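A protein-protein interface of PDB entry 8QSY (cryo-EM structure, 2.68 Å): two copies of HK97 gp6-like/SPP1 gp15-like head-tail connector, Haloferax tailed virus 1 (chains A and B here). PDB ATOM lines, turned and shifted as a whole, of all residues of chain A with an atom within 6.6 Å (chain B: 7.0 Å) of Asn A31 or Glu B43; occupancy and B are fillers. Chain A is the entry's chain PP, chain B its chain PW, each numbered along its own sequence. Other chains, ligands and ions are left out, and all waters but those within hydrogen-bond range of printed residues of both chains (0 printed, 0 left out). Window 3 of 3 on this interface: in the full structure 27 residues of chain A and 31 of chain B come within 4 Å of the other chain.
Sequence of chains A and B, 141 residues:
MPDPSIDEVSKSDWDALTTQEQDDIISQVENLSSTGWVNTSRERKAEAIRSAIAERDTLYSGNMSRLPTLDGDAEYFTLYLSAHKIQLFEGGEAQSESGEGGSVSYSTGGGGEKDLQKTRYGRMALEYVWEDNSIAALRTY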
ATOM      1  N   ILE A  26     -20.202 -10.179  -2.772  1.00  0.00           N
ATOM      2  CA  ILE A  26     -18.927 -10.345  -3.462  1.00  0.00           C
ATOM      3  C   ILE A  26     -17.780  -9.858  -2.575  1.00  0.00           C
ATOM      4  O   ILE A  26     -16.807 -10.583  -2.390  1.00  0.00           O
ATOM      5  CB  ILE A  26     -18.937  -9.661  -4.845  1.00  0.00           C
ATOM      6  CG1 ILE A  26     -19.835 -10.421  -5.822  1.00  0.00           C
ATOM      7  CG2 ILE A  26     -17.526  -9.514  -5.414  1.00  0.00           C
ATOM      8  CD1 ILE A  26     -20.308  -9.608  -7.005  1.00  0.00           C
ATOM      9  N   SER A  27     -17.916  -8.664  -1.981  1.00  0.00           N
ATOM     10  CA  SER A  27     -16.911  -8.097  -1.091  1.00  0.00           C
ATOM     11  C   SER A  27     -16.641  -9.020   0.092  1.00  0.00           C
ATOM     12  O   SER A  27     -15.488  -9.219   0.458  1.00  0.00           O
ATOM     13  CB  SER A  27     -17.294  -6.734  -0.606  1.00  0.00           C
ATOM     14  OG  SER A  27     -17.538  -5.869  -1.698  1.00  0.00           O
ATOM     15  N   GLN A  28     -17.689  -9.615   0.666  1.00  0.00           N
ATOM     16  CA  GLN A  28     -17.507 -10.572   1.741  1.00  0.00           C
ATOM     17  C   GLN A  28     -16.716 -11.802   1.277  1.00  0.00           C
ATOM     18  O   GLN A  28     -15.799 -12.232   1.969  1.00  0.00           O
ATOM     19  CB  GLN A  28     -18.843 -10.943   2.370  1.00  0.00           C
ATOM     20  CG  GLN A  28     -18.620 -11.697   3.667  1.00  0.00           C
ATOM     21  CD  GLN A  28     -19.873 -12.133   4.382  1.00  0.00           C
ATOM     22  OE1 GLN A  28     -20.977 -12.070   3.842  1.00  0.00           O
ATOM     23  NE2 GLN A  28     -19.706 -12.598   5.617  1.00  0.00           N
ATOM     24  N   VAL A  29     -17.031 -12.359   0.102  1.00  0.00           N
ATOM     25  CA  VAL A  29     -16.307 -13.516  -0.415  1.00  0.00           C
ATOM     26  C   VAL A  29     -14.833 -13.180  -0.638  1.00  0.00           C
ATOM     27  O   VAL A  29     -13.975 -13.962  -0.250  1.00  0.00           O
ATOM     28  CB  VAL A  29     -16.969 -14.118  -1.668  1.00  0.00           C
ATOM     29  CG1 VAL A  29     -16.102 -15.187  -2.321  1.00  0.00           C
ATOM     30  CG2 VAL A  29     -18.298 -14.740  -1.308  1.00  0.00           C
ATOM     31  N   GLU A  30     -14.525 -12.008  -1.201  1.00  0.00           N
ATOM     32  CA  GLU A  30     -13.153 -11.564  -1.417  1.00  0.00           C
ATOM     33  C   GLU A  30     -12.335 -11.455  -0.124  1.00  0.00           C
ATOM     34  O   GLU A  30     -11.108 -11.439  -0.186  1.00  0.00           O
ATOM     35  CB  GLU A  30     -13.143 -10.213  -2.121  1.00  0.00           C
ATOM     36  CG  GLU A  30     -13.622 -10.256  -3.556  1.00  0.00           C
ATOM     37  CD  GLU A  30     -13.630  -8.891  -4.227  1.00  0.00           C
ATOM     38  OE1 GLU A  30     -13.740  -7.870  -3.513  1.00  0.00           O
ATOM     39  OE2 GLU A  30     -13.512  -8.840  -5.466  1.00  0.00           O
ATOM     40  N   ASN A  31     -12.972 -11.378   1.048  1.00  0.00           N
ATOM     41  CA  ASN A  31     -12.237 -11.369   2.306  1.00  0.00           C
ATOM     42  C   ASN A  31     -11.608 -12.731   2.612  1.00  0.00           C
ATOM     43  O   ASN A  31     -10.692 -12.803   3.426  1.00  0.00           O
ATOM     44  CB  ASN A  31     -13.114 -10.931   3.478  1.00  0.00           C
ATOM     45  CG  ASN A  31     -13.611  -9.503   3.382  1.00  0.00           C
ATOM     46  OD1 ASN A  31     -13.024  -8.670   2.693  1.00  0.00           O
ATOM     47  ND2 ASN A  31     -14.685  -9.203   4.096  1.00  0.00           N
ATOM     48  N   LEU A  32     -12.061 -13.807   1.959  1.00  0.00           N
ATOM     49  CA  LEU A  32     -11.548 -15.147   2.229  1.00  0.00           C
ATOM     50  C   LEU A  32     -10.198 -15.424   1.554  1.00  0.00           C
ATOM     51  O   LEU A  32      -9.608 -16.470   1.797  1.00  0.00           O
ATOM     52  CB  LEU A  32     -12.593 -16.200   1.855  1.00  0.00           C
ATOM     53  CG  LEU A  32     -13.933 -16.101   2.577  1.00  0.00           C
ATOM     54  CD1 LEU A  32     -14.808 -17.282   2.193  1.00  0.00           C
ATOM     55  CD2 LEU A  32     -13.765 -16.049   4.085  1.00  0.00           C
ATOM     56  N   SER A  33      -9.671 -14.498   0.743  1.00  0.00           N
ATOM     57  CA  SER A  33      -8.305 -14.608   0.256  1.00  0.00           C
ATOM     58  C   SER A  33      -7.550 -13.309   0.511  1.00  0.00           C
ATOM     59  O   SER A  33      -8.068 -12.237   0.205  1.00  0.00           O
ATOM     60  CB  SER A  33      -8.273 -14.950  -1.201  1.00  0.00           C
ATOM     61  OG  SER A  33      -6.923 -14.966  -1.637  1.00  0.00           O
ATOM     62  N   SER A  34      -6.301 -13.419   0.979  1.00  0.00           N
ATOM     63  CA  SER A  34      -5.412 -12.281   1.200  1.00  0.00           C
ATOM     64  C   SER A  34      -5.115 -11.501  -0.089  1.00  0.00           C
ATOM     65  O   SER A  34      -4.792 -10.316  -0.032  1.00  0.00           O
ATOM     66  CB  SER A  34      -4.146 -12.719   1.875  1.00  0.00           C
ATOM     67  OG  SER A  34      -3.512 -13.713   1.086  1.00  0.00           O
ATOM     68  N   GLY A  36      -7.540 -11.361  -2.499  1.00  0.00           N
ATOM     69  CA  GLY A  36      -8.870 -10.915  -2.899  1.00  0.00           C
ATOM     70  C   GLY A  36      -9.294 -11.343  -4.307  1.00  0.00           C
ATOM     71  O   GLY A  36     -10.361 -10.932  -4.749  1.00  0.00           O
ATOM     72  N   TRP A  37      -8.474 -12.140  -5.017  1.00  0.00           N
ATOM     73  CA  TRP A  37      -8.666 -12.453  -6.434  1.00  0.00           C
ATOM     74  C   TRP A  37      -8.949 -11.188  -7.262  1.00  0.00           C
ATOM     75  O   TRP A  37      -9.853 -11.180  -8.106  1.00  0.00           O
ATOM     76  CB  TRP A  37      -9.752 -13.528  -6.626  1.00  0.00           C
ATOM     77  CG  TRP A  37      -9.610 -14.762  -5.785  1.00  0.00           C
ATOM     78  CD1 TRP A  37      -8.743 -15.794  -5.997  1.00  0.00           C
ATOM     79  CD2 TRP A  37     -10.376 -15.123  -4.610  1.00  0.00           C
ATOM     80  NE1 TRP A  37      -8.915 -16.757  -5.037  1.00  0.00           N
ATOM     81  CE2 TRP A  37      -9.912 -16.387  -4.168  1.00  0.00           C
ATOM     82  CE3 TRP A  37     -11.412 -14.519  -3.887  1.00  0.00           C
ATOM     83  CZ2 TRP A  37     -10.432 -17.026  -3.027  1.00  0.00           C
ATOM     84  CZ3 TRP A  37     -11.937 -15.148  -2.769  1.00  0.00           C
ATOM     85  CH2 TRP A  37     -11.447 -16.388  -2.338  1.00  0.00           C
ATOM     86  N   ILE B  26      -8.418  -9.170  17.560  1.00  0.00           N
ATOM     87  CA  ILE B  26      -7.543  -9.316  16.401  1.00  0.00           C
ATOM     88  C   ILE B  26      -6.079  -9.312  16.844  1.00  0.00           C
ATOM     89  O   ILE B  26      -5.331 -10.218  16.489  1.00  0.00           O
ATOM     90  CB  ILE B  26      -7.843  -8.245  15.331  1.00  0.00           C
ATOM     91  CG1 ILE B  26      -9.194  -8.506  14.663  1.00  0.00           C
ATOM     92  CG2 ILE B  26      -6.724  -8.173  14.289  1.00  0.00           C
ATOM     93  CD1 ILE B  26      -9.804  -7.307  13.975  1.00  0.00           C
ATOM     94  N   THR B  40      -1.779  -9.072   5.473  1.00  0.00           N
ATOM     95  CA  THR B  40      -3.207  -9.359   5.336  1.00  0.00           C
ATOM     96  C   THR B  40      -3.998  -8.241   6.018  1.00  0.00           C
ATOM     97  O   THR B  40      -3.715  -7.893   7.162  1.00  0.00           O
ATOM     98  CB  THR B  40      -3.540 -10.757   5.886  1.00  0.00           C
ATOM     99  OG1 THR B  40      -3.184 -11.727   4.907  1.00  0.00           O
ATOM    100  CG2 THR B  40      -5.007 -11.000   6.168  1.00  0.00           C
ATOM    101  N   SER B  41      -5.007  -7.690   5.324  1.00  0.00           N
ATOM    102  CA  SER B  41      -5.739  -6.519   5.802  1.00  0.00           C
ATOM    103  C   SER B  41      -6.703  -6.847   6.949  1.00  0.00           C
ATOM    104  O   SER B  41      -7.068  -8.001   7.163  1.00  0.00           O
ATOM    105  CB  SER B  41      -6.441  -5.819   4.664  1.00  0.00           C
ATOM    106  OG  SER B  41      -7.601  -6.533   4.246  1.00  0.00           O
ATOM    107  N   ARG B  42      -7.165  -5.811   7.664  1.00  0.00           N
ATOM    108  CA  ARG B  42      -8.043  -5.954   8.817  1.00  0.00           C
ATOM    109  C   ARG B  42      -9.307  -6.756   8.499  1.00  0.00           C
ATOM    110  O   ARG B  42      -9.669  -7.636   9.277  1.00  0.00           O
ATOM    111  CB  ARG B  42      -8.404  -4.587   9.392  1.00  0.00           C
ATOM    112  CG  ARG B  42      -9.179  -4.707  10.690  1.00  0.00           C
ATOM    113  CD  ARG B  42      -9.825  -3.416  11.152  1.00  0.00           C
ATOM    114  NE  ARG B  42     -10.516  -3.629  12.408  1.00  0.00           N
ATOM    115  CZ  ARG B  42     -11.763  -4.064  12.555  1.00  0.00           C
ATOM    116  NH1 ARG B  42     -12.223  -4.220  13.777  1.00  0.00           N
ATOM    117  NH2 ARG B  42     -12.549  -4.343  11.529  1.00  0.00           N
ATOM    118  N   GLU B  43      -9.970  -6.464   7.372  1.00  0.00           N
ATOM    119  CA  GLU B  43     -11.251  -7.072   7.019  1.00  0.00           C
ATOM    120  C   GLU B  43     -11.158  -8.599   6.953  1.00  0.00           C
ATOM    121  O   GLU B  43     -12.113  -9.303   7.272  1.00  0.00           O
ATOM    122  CB  GLU B  43     -11.766  -6.580   5.666  1.00  0.00           C
ATOM    123  CG  GLU B  43     -11.826  -5.070   5.522  1.00  0.00           C
ATOM    124  CD  GLU B  43     -10.609  -4.446   4.856  1.00  0.00           C
ATOM    125  OE1 GLU B  43      -9.488  -4.942   5.087  1.00  0.00           O
ATOM    126  OE2 GLU B  43     -10.789  -3.462   4.108  1.00  0.00           O
ATOM    127  N   ARG B  44      -9.990  -9.100   6.553  1.00  0.00           N
ATOM    128  CA  ARG B  44      -9.732 -10.518   6.365  1.00  0.00           C
ATOM    129  C   ARG B  44      -9.495 -11.217   7.699  1.00  0.00           C
ATOM    130  O   ARG B  44     -10.014 -12.306   7.918  1.00  0.00           O
ATOM    131  CB  ARG B  44      -8.581 -10.679   5.381  1.00  0.00           C
ATOM    132  CG  ARG B  44      -8.949 -10.021   4.066  1.00  0.00           C
ATOM    133  CD  ARG B  44      -8.002 -10.254   2.919  1.00  0.00           C
ATOM    134  NE  ARG B  44      -8.663 -10.018   1.644  1.00  0.00           N
ATOM    135  CZ  ARG B  44      -8.914  -8.836   1.083  1.00  0.00           C
ATOM    136  NH1 ARG B  44      -9.524  -8.800  -0.087  1.00  0.00           N
ATOM    137  NH2 ARG B  44      -8.567  -7.703   1.662  1.00  0.00           N
ATOM    138  N   LYS B  45      -8.782 -10.560   8.615  1.00  0.00           N
ATOM    139  CA  LYS B  45      -8.628 -11.036   9.981  1.00  0.00           C
ATOM    140  C   LYS B  45      -9.960 -11.023  10.726  1.00  0.00           C
ATOM    141  O   LYS B  45     -10.298 -12.004  11.380  1.00  0.00           O
ATOM    142  CB  LYS B  45      -7.478 -10.298  10.662  1.00  0.00           C
ATOM    143  CG  LYS B  45      -6.145 -10.801  10.142  1.00  0.00           C
ATOM    144  CD  LYS B  45      -4.915 -10.083  10.660  1.00  0.00           C
ATOM    145  CE  LYS B  45      -4.694  -8.735  10.009  1.00  0.00           C
ATOM    146  NZ  LYS B  45      -3.328  -8.215  10.259  1.00  0.00           N
ATOM    147  N   ALA B  46     -10.765  -9.971  10.543  1.00  0.00           N
ATOM    148  CA  ALA B  46     -12.123  -9.911  11.065  1.00  0.00           C
ATOM    149  C   ALA B  46     -12.994 -11.041  10.496  1.00  0.00           C
ATOM    150  O   ALA B  46     -13.675 -11.729  11.256  1.00  0.00           O
ATOM    151  CB  ALA B  46     -12.687  -8.540  10.801  1.00  0.00           C
ATOM    152  N   GLU B  47     -12.940 -11.291   9.180  1.00  0.00           N
ATOM    153  CA  GLU B  47     -13.694 -12.370   8.547  1.00  0.00           C
ATOM    154  C   GLU B  47     -13.294 -13.741   9.104  1.00  0.00           C
ATOM    155  O   GLU B  47     -14.156 -14.567   9.403  1.00  0.00           O
ATOM    156  CB  GLU B  47     -13.513 -12.333   7.031  1.00  0.00           C
ATOM    157  CG  GLU B  47     -14.612 -13.060   6.276  1.00  0.00           C
ATOM    158  CD  GLU B  47     -15.933 -12.305   6.223  1.00  0.00           C
ATOM    159  OE1 GLU B  47     -15.920 -11.121   5.827  1.00  0.00           O
ATOM    160  OE2 GLU B  47     -16.967 -12.895   6.585  1.00  0.00           O
ATOM    161  N   ALA B  48     -11.987 -13.979   9.268  1.00  0.00           N
ATOM    162  CA  ALA B  48     -11.461 -15.219   9.820  1.00  0.00           C
ATOM    163  C   ALA B  48     -11.957 -15.455  11.253  1.00  0.00           C
ATOM    164  O   ALA B  48     -12.389 -16.557  11.568  1.00  0.00           O
ATOM    165  CB  ALA B  48      -9.959 -15.200   9.757  1.00  0.00           C
ATOM    166  N   PHE B  89      -6.213 -18.178   4.387  1.00  0.00           N
ATOM    167  CA  PHE B  89      -6.452 -17.001   3.556  1.00  0.00           C
ATOM    168  C   PHE B  89      -5.139 -16.487   2.946  1.00  0.00           C
ATOM    169  O   PHE B  89      -5.149 -15.935   1.847  1.00  0.00           O
ATOM    170  CB  PHE B  89      -7.171 -15.901   4.344  1.00  0.00           C
ATOM    171  CG  PHE B  89      -8.538 -16.188   4.929  1.00  0.00           C
ATOM    172  CD1 PHE B  89      -9.154 -17.436   4.840  1.00  0.00           C
ATOM    173  CD2 PHE B  89      -9.217 -15.181   5.609  1.00  0.00           C
ATOM    174  CE1 PHE B  89     -10.398 -17.665   5.426  1.00  0.00           C
ATOM    175  CE2 PHE B  89     -10.464 -15.405   6.180  1.00  0.00           C
ATOM    176  CZ  PHE B  89     -11.048 -16.648   6.096  1.00  0.00           C
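The side-chain carboxylate of Glu B47 is in hydrogen-bond range of the side-chain amide nitrogen of Gln A28 (2.9 Å).
The guanidinium group (NH1) of Arg B44 is in hydrogen-bond range of the backbone carbonyl oxygen (O) of Glu A30, 3.1 Å away.
OE1 of Glu B47 sits at hydrogen-bond distance from ND2 of Asn A31 (2.9 Å).
The backbone carbonyl oxygen of Ser A33 lies within hydrogen-bond range of the guanidinium group of Arg B44.
OG of Ser A34 lies within hydrogen-bond range of O of Phe B89.
The side-chain amide oxygen of Asn A31 lies close to the backbone carbonyl oxygen of Ser A27 (3.4 Å).
NZ of Lys B45 lies close to O of Thr B40, at 3.1 Å.
The side-chain hydroxyl (OG) of Ser B41 sits at hydrogen-bond distance from the side-chain carboxylate (OE1) of Glu B43.
The guanidinium group (NH2) of Arg B44 sits at hydrogen-bond distance from the side-chain hydroxyl (OG) of Ser B41.
Asn A31 touches Glu B43.
O of Asn A31 touches CG of Arg B44, 3.3 Å away.
Phe B89 touches Asn A31 (CD2 to O, 3.5 Å).
Leu A32 touches Glu B47.
Phe B89 touches Leu A32.
Phe B89 touches Ser A33.
Ser A34 touches Thr B40 (CB to OG1, 3.3 Å).
Ser A34 touches Arg B44.
Gly A36 touches Arg B44.
Glu B43 touches one residue of chain A.
Of the printed residues of chain B, Gly A36 touches Arg B44.
Of the printed residues of chain A, Phe B89 touches Asn A31 (3.5 Å), Leu A32 (3.2 Å), Ser A33 (3.8 Å) and Ser A34 (2.9 Å).
Of the printed residues of chain B, Ser A33 touches Arg B44 (2.7 Å) and Phe B89 (3.8 Å).
Of the printed residues of chain B, Glu A30 touches Arg B44.
Of the printed residues of chain B, Leu A32 touches Glu B47 and Phe B89.
The nearest printed residue of chain A that does not touch Glu B43 is Ser A27 (6.9 Å).
The nearest printed residue of chain A that does not touch Glu B47 is Ser A27 (5.7 Å).
Printed residues of chain A that touch a printed residue of chain B: Gln A28, Glu A30, Asn A31, Leu A32, Ser A33, Ser A34 and Gly A36.
Hydrophobic or aromatic side chains of chain A that line the printed part of chain B: Leu A32.
Among the printed residues, 14 pairs touch across the chains.
Among the printed residues, no Asp or Glu carboxylate lies within 4 Å of a Lys or Arg side-chain nitrogen of the other chain.
1 position is printed for both chains.
Of the 14 pairs that touch across the chains among the printed residues, none has its exchanged pair printed and touching as well.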
